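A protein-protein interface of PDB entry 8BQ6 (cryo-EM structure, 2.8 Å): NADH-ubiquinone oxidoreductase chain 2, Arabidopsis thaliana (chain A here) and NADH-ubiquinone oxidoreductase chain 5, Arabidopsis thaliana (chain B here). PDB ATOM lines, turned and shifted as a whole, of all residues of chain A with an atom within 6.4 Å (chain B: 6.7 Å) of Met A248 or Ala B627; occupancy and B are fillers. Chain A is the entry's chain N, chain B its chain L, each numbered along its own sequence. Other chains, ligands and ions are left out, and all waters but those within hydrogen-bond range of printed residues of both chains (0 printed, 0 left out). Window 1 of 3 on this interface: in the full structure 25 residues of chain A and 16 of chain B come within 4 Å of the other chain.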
ATOM      1  N   LEU A 182      13.775  15.738 -17.326  1.00  0.00           N
ATOM      2  CA  LEU A 182      14.505  15.404 -18.576  1.00  0.00           C
ATOM      3  C   LEU A 182      15.680  14.483 -18.247  1.00  0.00           C
ATOM      4  O   LEU A 182      15.964  13.597 -19.062  1.00  0.00           O
ATOM      5  CB  LEU A 182      14.937  16.711 -19.243  1.00  0.00           C
ATOM      6  CG  LEU A 182      13.783  17.660 -19.567  1.00  0.00           C
ATOM      7  CD1 LEU A 182      14.288  18.989 -20.097  1.00  0.00           C
ATOM      8  CD2 LEU A 182      12.802  17.027 -20.537  1.00  0.00           C
ATOM      9  N   ALA A 243      24.148  17.452 -26.802  1.00  0.00           N
ATOM     10  CA  ALA A 243      24.121  17.457 -28.254  1.00  0.00           C
ATOM     11  C   ALA A 243      22.687  17.567 -28.756  1.00  0.00           C
ATOM     12  O   ALA A 243      21.776  16.926 -28.225  1.00  0.00           O
ATOM     13  CB  ALA A 243      24.776  16.195 -28.813  1.00  0.00           C
ATOM     14  N   PRO A 245      19.629  16.658 -31.027  1.00  0.00           N
ATOM     15  CA  PRO A 245      18.403  17.264 -30.510  1.00  0.00           C
ATOM     16  C   PRO A 245      18.109  16.899 -29.064  1.00  0.00           C
ATOM     17  O   PRO A 245      16.946  16.871 -28.684  1.00  0.00           O
ATOM     18  CB  PRO A 245      17.335  16.674 -31.432  1.00  0.00           C
ATOM     19  CG  PRO A 245      17.858  15.286 -31.755  1.00  0.00           C
ATOM     20  CD  PRO A 245      19.358  15.299 -31.521  1.00  0.00           C
ATOM     21  N   PHE A 246      19.100  16.592 -28.232  1.00  0.00           N
ATOM     22  CA  PHE A 246      18.864  16.259 -26.827  1.00  0.00           C
ATOM     23  C   PHE A 246      19.430  17.319 -25.895  1.00  0.00           C
ATOM     24  O   PHE A 246      19.961  17.014 -24.826  1.00  0.00           O
ATOM     25  CB  PHE A 246      19.437  14.886 -26.505  1.00  0.00           C
ATOM     26  CG  PHE A 246      19.071  13.839 -27.508  1.00  0.00           C
ATOM     27  CD1 PHE A 246      17.847  13.201 -27.435  1.00  0.00           C
ATOM     28  CD2 PHE A 246      19.939  13.497 -28.525  1.00  0.00           C
ATOM     29  CE1 PHE A 246      17.496  12.242 -28.357  1.00  0.00           C
ATOM     30  CE2 PHE A 246      19.592  12.533 -29.447  1.00  0.00           C
ATOM     31  CZ  PHE A 246      18.368  11.906 -29.363  1.00  0.00           C
ATOM     32  N   HIS A 247      19.285  18.585 -26.278  1.00  0.00           N
ATOM     33  CA  HIS A 247      20.019  19.693 -25.687  1.00  0.00           C
ATOM     34  C   HIS A 247      19.157  20.701 -24.944  1.00  0.00           C
ATOM     35  O   HIS A 247      19.703  21.504 -24.187  1.00  0.00           O
ATOM     36  CB  HIS A 247      20.756  20.463 -26.781  1.00  0.00           C
ATOM     37  CG  HIS A 247      19.821  21.185 -27.695  1.00  0.00           C
ATOM     38  ND1 HIS A 247      19.111  20.541 -28.685  1.00  0.00           N
ATOM     39  CD2 HIS A 247      19.404  22.473 -27.709  1.00  0.00           C
ATOM     40  CE1 HIS A 247      18.335  21.412 -29.303  1.00  0.00           C
ATOM     41  NE2 HIS A 247      18.491  22.591 -28.727  1.00  0.00           N
ATOM     42  N   MET A 248      17.841  20.723 -25.173  1.00  0.00           N
ATOM     43  CA  MET A 248      17.056  21.878 -24.744  1.00  0.00           C
ATOM     44  C   MET A 248      16.980  22.015 -23.231  1.00  0.00           C
ATOM     45  O   MET A 248      16.600  23.082 -22.741  1.00  0.00           O
ATOM     46  CB  MET A 248      15.649  21.838 -25.346  1.00  0.00           C
ATOM     47  CG  MET A 248      15.597  21.221 -26.720  1.00  0.00           C
ATOM     48  SD  MET A 248      13.957  21.106 -27.451  1.00  0.00           S
ATOM     49  CE  MET A 248      13.517  22.831 -27.599  1.00  0.00           C
ATOM     50  N   TRP A 249      17.387  20.996 -22.493  1.00  0.00           N
ATOM     51  CA  TRP A 249      17.459  21.156 -21.023  1.00  0.00           C
ATOM     52  C   TRP A 249      18.609  22.091 -20.664  1.00  0.00           C
ATOM     53  O   TRP A 249      18.467  22.818 -19.676  1.00  0.00           O
ATOM     54  CB  TRP A 249      17.692  19.795 -20.364  1.00  0.00           C
ATOM     55  CG  TRP A 249      19.045  19.208 -20.628  1.00  0.00           C
ATOM     56  CD1 TRP A 249      19.428  18.486 -21.718  1.00  0.00           C
ATOM     57  CD2 TRP A 249      20.207  19.300 -19.783  1.00  0.00           C
ATOM     58  NE1 TRP A 249      20.740  18.114 -21.607  1.00  0.00           N
ATOM     59  CE2 TRP A 249      21.246  18.605 -20.435  1.00  0.00           C
ATOM     60  CE3 TRP A 249      20.473  19.906 -18.551  1.00  0.00           C
ATOM     61  CZ2 TRP A 249      22.521  18.488 -19.885  1.00  0.00           C
ATOM     62  CZ3 TRP A 249      21.737  19.801 -18.016  1.00  0.00           C
ATOM     63  CH2 TRP A 249      22.746  19.098 -18.674  1.00  0.00           C
ATOM     64  N   ALA A 250      19.676  22.125 -21.468  1.00  0.00           N
ATOM     65  CA  ALA A 250      20.890  22.822 -21.049  1.00  0.00           C
ATOM     66  C   ALA A 250      20.728  24.332 -20.919  1.00  0.00           C
ATOM     67  O   ALA A 250      21.075  24.866 -19.856  1.00  0.00           O
ATOM     68  CB  ALA A 250      22.045  22.462 -21.987  1.00  0.00           C
ATOM     69  N   PRO A 251      20.243  25.080 -21.921  1.00  0.00           N
ATOM     70  CA  PRO A 251      20.175  26.544 -21.735  1.00  0.00           C
ATOM     71  C   PRO A 251      19.292  26.968 -20.570  1.00  0.00           C
ATOM     72  O   PRO A 251      19.653  27.888 -19.819  1.00  0.00           O
ATOM     73  CB  PRO A 251      19.633  27.051 -23.080  1.00  0.00           C
ATOM     74  CG  PRO A 251      19.794  25.923 -24.031  1.00  0.00           C
ATOM     75  CD  PRO A 251      19.705  24.676 -23.230  1.00  0.00           C
ATOM     76  N   ASP A 252      18.163  26.287 -20.370  1.00  0.00           N
ATOM     77  CA  ASP A 252      17.254  26.668 -19.295  1.00  0.00           C
ATOM     78  C   ASP A 252      17.861  26.380 -17.926  1.00  0.00           C
ATOM     79  O   ASP A 252      17.735  27.190 -16.999  1.00  0.00           O
ATOM     80  CB  ASP A 252      15.920  25.940 -19.454  1.00  0.00           C
ATOM     81  CG  ASP A 252      15.036  26.563 -20.522  1.00  0.00           C
ATOM     82  OD1 ASP A 252      15.485  27.504 -21.208  1.00  0.00           O
ATOM     83  OD2 ASP A 252      13.875  26.130 -20.656  1.00  0.00           O
ATOM     84  N   ILE A 253      18.541  25.244 -17.796  1.00  0.00           N
ATOM     85  CA  ILE A 253      19.143  24.861 -16.484  1.00  0.00           C
ATOM     86  C   ILE A 253      20.358  25.756 -16.241  1.00  0.00           C
ATOM     87  O   ILE A 253      20.531  26.215 -15.103  1.00  0.00           O
ATOM     88  CB  ILE A 253      19.480  23.353 -16.435  1.00  0.00           C
ATOM     89  CG1 ILE A 253      18.291  22.525 -15.941  1.00  0.00           C
ATOM     90  CG2 ILE A 253      20.721  23.077 -15.598  1.00  0.00           C
ATOM     91  CD1 ILE A 253      17.054  22.615 -16.798  1.00  0.00           C
ATOM     92  N   ARG A 317      22.794  32.716 -21.334  1.00  0.00           N
ATOM     93  CA  ARG A 317      22.247  31.942 -22.446  1.00  0.00           C
ATOM     94  C   ARG A 317      23.228  31.874 -23.605  1.00  0.00           C
ATOM     95  O   ARG A 317      23.360  30.832 -24.265  1.00  0.00           O
ATOM     96  CB  ARG A 317      20.938  32.551 -22.932  1.00  0.00           C
ATOM     97  CG  ARG A 317      19.841  32.489 -21.976  1.00  0.00           C
ATOM     98  CD  ARG A 317      18.481  32.613 -22.642  1.00  0.00           C
ATOM     99  NE  ARG A 317      18.037  31.354 -23.219  1.00  0.00           N
ATOM    100  CZ  ARG A 317      17.439  30.393 -22.531  1.00  0.00           C
ATOM    101  NH1 ARG A 317      17.261  30.487 -21.223  1.00  0.00           N
ATOM    102  NH2 ARG A 317      16.994  29.317 -23.172  1.00  0.00           N
ATOM    103  N   ILE A 324      27.107  24.416 -26.441  1.00  0.00           N
ATOM    104  CA  ILE A 324      26.468  23.427 -27.316  1.00  0.00           C
ATOM    105  C   ILE A 324      27.187  23.357 -28.666  1.00  0.00           C
ATOM    106  O   ILE A 324      27.534  22.270 -29.166  1.00  0.00           O
ATOM    107  CB  ILE A 324      24.973  23.758 -27.484  1.00  0.00           C
ATOM    108  CG1 ILE A 324      24.216  23.490 -26.182  1.00  0.00           C
ATOM    109  CG2 ILE A 324      24.365  22.971 -28.627  1.00  0.00           C
ATOM    110  CD1 ILE A 324      22.812  24.038 -26.177  1.00  0.00           C
ATOM    111  N   LEU B 616      12.098  27.884 -30.754  1.00  0.00           N
ATOM    112  CA  LEU B 616      12.010  26.458 -30.453  1.00  0.00           C
ATOM    113  C   LEU B 616      12.167  26.197 -28.962  1.00  0.00           C
ATOM    114  O   LEU B 616      11.480  25.338 -28.396  1.00  0.00           O
ATOM    115  CB  LEU B 616      13.083  25.705 -31.230  1.00  0.00           C
ATOM    116  CG  LEU B 616      12.666  24.967 -32.494  1.00  0.00           C
ATOM    117  CD1 LEU B 616      11.915  25.899 -33.422  1.00  0.00           C
ATOM    118  CD2 LEU B 616      13.913  24.441 -33.163  1.00  0.00           C
ATOM    119  N   GLN B 617      13.083  26.916 -28.315  1.00  0.00           N
ATOM    120  CA  GLN B 617      13.251  26.865 -26.868  1.00  0.00           C
ATOM    121  C   GLN B 617      12.093  27.584 -26.197  1.00  0.00           C
ATOM    122  O   GLN B 617      12.257  28.687 -25.668  1.00  0.00           O
ATOM    123  CB  GLN B 617      14.582  27.501 -26.464  1.00  0.00           C
ATOM    124  CG  GLN B 617      15.043  27.186 -25.051  1.00  0.00           C
ATOM    125  CD  GLN B 617      15.675  25.822 -24.934  1.00  0.00           C
ATOM    126  OE1 GLN B 617      15.973  25.177 -25.936  1.00  0.00           O
ATOM    127  NE2 GLN B 617      15.892  25.375 -23.704  1.00  0.00           N
ATOM    128  N   SER B 618      10.917  26.959 -26.209  1.00  0.00           N
ATOM    129  CA  SER B 618       9.683  27.647 -25.859  1.00  0.00           C
ATOM    130  C   SER B 618       9.516  27.880 -24.364  1.00  0.00           C
ATOM    131  O   SER B 618       8.645  28.663 -23.970  1.00  0.00           O
ATOM    132  CB  SER B 618       8.485  26.857 -26.388  1.00  0.00           C
ATOM    133  OG  SER B 618       8.405  25.584 -25.775  1.00  0.00           O
ATOM    134  N   PHE B 620       8.629  25.423 -22.346  1.00  0.00           N
ATOM    135  CA  PHE B 620       7.723  24.384 -21.886  1.00  0.00           C
ATOM    136  C   PHE B 620       8.493  23.077 -21.781  1.00  0.00           C
ATOM    137  O   PHE B 620       9.136  22.650 -22.747  1.00  0.00           O
ATOM    138  CB  PHE B 620       6.535  24.249 -22.834  1.00  0.00           C
ATOM    139  CG  PHE B 620       5.580  25.396 -22.750  1.00  0.00           C
ATOM    140  CD1 PHE B 620       4.639  25.459 -21.741  1.00  0.00           C
ATOM    141  CD2 PHE B 620       5.652  26.431 -23.658  1.00  0.00           C
ATOM    142  CE1 PHE B 620       3.770  26.522 -21.655  1.00  0.00           C
ATOM    143  CE2 PHE B 620       4.788  27.495 -23.577  1.00  0.00           C
ATOM    144  CZ  PHE B 620       3.844  27.541 -22.574  1.00  0.00           C
ATOM    145  N   TYR B 622       7.294  20.190 -21.626  1.00  0.00           N
ATOM    146  CA  TYR B 622       6.693  19.167 -22.471  1.00  0.00           C
ATOM    147  C   TYR B 622       7.332  19.156 -23.853  1.00  0.00           C
ATOM    148  O   TYR B 622       7.495  18.094 -24.462  1.00  0.00           O
ATOM    149  CB  TYR B 622       5.188  19.390 -22.569  1.00  0.00           C
ATOM    150  CG  TYR B 622       4.500  18.499 -23.571  1.00  0.00           C
ATOM    151  CD1 TYR B 622       4.205  17.179 -23.266  1.00  0.00           C
ATOM    152  CD2 TYR B 622       4.140  18.979 -24.820  1.00  0.00           C
ATOM    153  CE1 TYR B 622       3.566  16.365 -24.175  1.00  0.00           C
ATOM    154  CE2 TYR B 622       3.510  18.169 -25.736  1.00  0.00           C
ATOM    155  CZ  TYR B 622       3.225  16.865 -25.409  1.00  0.00           C
ATOM    156  OH  TYR B 622       2.593  16.058 -26.321  1.00  0.00           O
ATOM    157  N   HIS B 623       7.705  20.332 -24.360  1.00  0.00           N
ATOM    158  CA  HIS B 623       8.352  20.398 -25.664  1.00  0.00           C
ATOM    159  C   HIS B 623       9.735  19.766 -25.628  1.00  0.00           C
ATOM    160  O   HIS B 623      10.176  19.170 -26.613  1.00  0.00           O
ATOM    161  CB  HIS B 623       8.436  21.847 -26.134  1.00  0.00           C
ATOM    162  CG  HIS B 623       7.164  22.361 -26.728  1.00  0.00           C
ATOM    163  ND1 HIS B 623       6.731  23.655 -26.552  1.00  0.00           N
ATOM    164  CD2 HIS B 623       6.234  21.755 -27.504  1.00  0.00           C
ATOM    165  CE1 HIS B 623       5.588  23.827 -27.190  1.00  0.00           C
ATOM    166  NE2 HIS B 623       5.265  22.688 -27.776  1.00  0.00           N
ATOM    167  N   TYR B 624      10.429  19.872 -24.497  1.00  0.00           N
ATOM    168  CA  TYR B 624      11.767  19.298 -24.398  1.00  0.00           C
ATOM    169  C   TYR B 624      11.703  17.776 -24.383  1.00  0.00           C
ATOM    170  O   TYR B 624      12.499  17.100 -25.049  1.00  0.00           O
ATOM    171  CB  TYR B 624      12.462  19.829 -23.145  1.00  0.00           C
ATOM    172  CG  TYR B 624      12.566  21.339 -23.088  1.00  0.00           C
ATOM    173  CD1 TYR B 624      12.234  22.126 -24.185  1.00  0.00           C
ATOM    174  CD2 TYR B 624      12.955  21.979 -21.924  1.00  0.00           C
ATOM    175  CE1 TYR B 624      12.310  23.494 -24.131  1.00  0.00           C
ATOM    176  CE2 TYR B 624      13.035  23.352 -21.861  1.00  0.00           C
ATOM    177  CZ  TYR B 624      12.711  24.103 -22.968  1.00  0.00           C
ATOM    178  OH  TYR B 624      12.788  25.473 -22.913  1.00  0.00           O
ATOM    179  N   ALA B 625      10.740  17.223 -23.642  1.00  0.00           N
ATOM    180  CA  ALA B 625      10.517  15.784 -23.655  1.00  0.00           C
ATOM    181  C   ALA B 625      10.053  15.310 -25.025  1.00  0.00           C
ATOM    182  O   ALA B 625      10.483  14.255 -25.502  1.00  0.00           O
ATOM    183  CB  ALA B 625       9.499  15.406 -22.583  1.00  0.00           C
ATOM    184  N   PHE B 626       9.168  16.074 -25.666  1.00  0.00           N
ATOM    185  CA  PHE B 626       8.716  15.723 -27.005  1.00  0.00           C
ATOM    186  C   PHE B 626       9.877  15.722 -27.992  1.00  0.00           C
ATOM    187  O   PHE B 626       9.968  14.843 -28.851  1.00  0.00           O
ATOM    188  CB  PHE B 626       7.624  16.692 -27.457  1.00  0.00           C
ATOM    189  CG  PHE B 626       6.868  16.236 -28.669  1.00  0.00           C
ATOM    190  CD1 PHE B 626       6.768  14.893 -28.988  1.00  0.00           C
ATOM    191  CD2 PHE B 626       6.306  17.163 -29.528  1.00  0.00           C
ATOM    192  CE1 PHE B 626       6.082  14.485 -30.118  1.00  0.00           C
ATOM    193  CE2 PHE B 626       5.625  16.760 -30.657  1.00  0.00           C
ATOM    194  CZ  PHE B 626       5.515  15.422 -30.953  1.00  0.00           C
ATOM    195  N   ALA B 627      10.778  16.701 -27.879  1.00  0.00           N
ATOM    196  CA  ALA B 627      11.958  16.734 -28.734  1.00  0.00           C
ATOM    197  C   ALA B 627      12.860  15.534 -28.485  1.00  0.00           C
ATOM    198  O   ALA B 627      13.382  14.935 -29.433  1.00  0.00           O
ATOM    199  CB  ALA B 627      12.729  18.032 -28.513  1.00  0.00           C
ATOM    200  N   MET B 628      13.066  15.171 -27.217  1.00  0.00           N
ATOM    201  CA  MET B 628      13.864  13.982 -26.924  1.00  0.00           C
ATOM    202  C   MET B 628      13.230  12.734 -27.525  1.00  0.00           C
ATOM    203  O   MET B 628      13.918  11.895 -28.121  1.00  0.00           O
ATOM    204  CB  MET B 628      14.029  13.821 -25.414  1.00  0.00           C
ATOM    205  CG  MET B 628      14.973  14.822 -24.789  1.00  0.00           C
ATOM    206  SD  MET B 628      14.951  14.769 -22.987  1.00  0.00           S
ATOM    207  CE  MET B 628      15.365  13.055 -22.683  1.00  0.00           C
ATOM    208  N   LEU B 629      11.912  12.603 -27.383  1.00  0.00           N
ATOM    209  CA  LEU B 629      11.207  11.446 -27.917  1.00  0.00           C
ATOM    210  C   LEU B 629      11.282  11.406 -29.436  1.00  0.00           C
ATOM    211  O   LEU B 629      11.436  10.334 -30.030  1.00  0.00           O
ATOM    212  CB  LEU B 629       9.757  11.478 -27.448  1.00  0.00           C
ATOM    213  CG  LEU B 629       8.883  10.285 -27.802  1.00  0.00           C
ATOM    214  CD1 LEU B 629       9.617   8.990 -27.520  1.00  0.00           C
ATOM    215  CD2 LEU B 629       7.609  10.367 -26.995  1.00  0.00           C
ATOM    216  N   LEU B 630      11.160  12.566 -30.079  1.00  0.00           N
ATOM    217  CA  LEU B 630      11.262  12.636 -31.531  1.00  0.00           C
ATOM    218  C   LEU B 630      12.660  12.273 -32.001  1.00  0.00           C
ATOM    219  O   LEU B 630      12.820  11.605 -33.024  1.00  0.00           O
ATOM    220  CB  LEU B 630      10.888  14.034 -32.012  1.00  0.00           C
ATOM    221  CG  LEU B 630       9.403  14.376 -31.999  1.00  0.00           C
ATOM    222  CD1 LEU B 630       9.225  15.812 -32.441  1.00  0.00           C
ATOM    223  CD2 LEU B 630       8.623  13.429 -32.893  1.00  0.00           C
ATOM    224  N   GLY B 631      13.686  12.718 -31.276  1.00  0.00           N
ATOM    225  CA  GLY B 631      15.040  12.316 -31.615  1.00  0.00           C
ATOM    226  C   GLY B 631      15.247  10.820 -31.491  1.00  0.00           C
ATOM    227  O   GLY B 631      15.865  10.192 -32.354  1.00  0.00           O
ATOM    228  N   LEU B 632      14.726  10.226 -30.415  1.00  0.00           N
ATOM    229  CA  LEU B 632      14.788   8.773 -30.265  1.00  0.00           C
ATOM    230  C   LEU B 632      14.087   8.064 -31.418  1.00  0.00           C
ATOM    231  O   LEU B 632      14.647   7.141 -32.029  1.00  0.00           O
ATOM    232  CB  LEU B 632      14.165   8.371 -28.931  1.00  0.00           C
ATOM    233  CG  LEU B 632      14.290   6.924 -28.466  1.00  0.00           C
ATOM    234  CD1 LEU B 632      15.742   6.512 -28.339  1.00  0.00           C
ATOM    235  CD2 LEU B 632      13.573   6.785 -27.144  1.00  0.00           C
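OH of Tyr B624 sits at hydrogen-bond distance from OD2 of Asp A252 (2.6 Å).
The side-chain carboxylate (OD1) of Asp A252 lies within hydrogen-bond range of the side-chain amide nitrogen (NE2) of Gln B617 (3.3 Å).
NE2 of Gln B617 lies within hydrogen-bond range of O of Met A248.
NE2 of Gln B617 lies within hydrogen-bond range of OH of Tyr B624, at 3.2 Å.
The guanidinium group (NH2) of Arg A317 is in salt-bridge range of the side-chain carboxylate (OD1) of Asp A252 (3.1 Å).
The backbone carbonyl oxygen of Phe A246 lies close to the indole nitrogen of Trp A249 (3.5 Å).
Among the printed residues, pairs that only touch across the chains: Met A248 with Leu B616, Arg A317 with Gln B617, Met A248 with Ala B627, Phe A246 with Met B628, Met A248 with Tyr B624, Leu A182 with Tyr B624, Leu A182 with Met B628, Leu A182 with Ala B625, Pro A251 with Gln B617, Phe A246 with Gly B631 and Phe A246 with Leu B632.
Of chain B, only Leu B616, Gln B617, Tyr B624 and Ala B627 come within 4 Å of Met A248.
Printed residues of chain B within 4 Å of Asp A252: Gln B617 (3.3 Å) and Tyr B624 (2.6 Å).
Of the printed residues of chain A, Tyr B624 touches Leu A182 (3.7 Å), Met A248 (3.6 Å) and Asp A252 (2.6 Å).
Of chain A, only Met A248 (3.5 Å) comes within 4 Å of Ala B627.
Printed residues of chain A within 4 Å of Met B628: Leu A182 and Phe A246.
Leu B630 touches none of the printed residues of chain A.
The nearest residue of chain A that does not touch Ala B627 is Pro A245 (4.1 Å).
Of the 13 printed residues of chain A, 6 touch a printed residue of chain B.
Hydrophobic or aromatic side chains of chain A within 4 Å of the printed part of chain B: Leu A182, Phe A246, Met A248 and Pro A251.
Printed residues of chain B that touch a printed residue of chain A: Leu B616, Gln B617, Tyr B624, Ala B625, Ala B627, Met B628, Gly B631 and Leu B632.
Hydrophobic or aromatic side chains of chain B within 4 Å of the printed part of chain A: Tyr B624, Ala B627 and Met B628.
Among the printed residues, 14 pairs touch across the chains.
Among the printed residues, no Asp or Glu carboxylate lies within 4 Å of a Lys or Arg side-chain nitrogen of the other chain.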
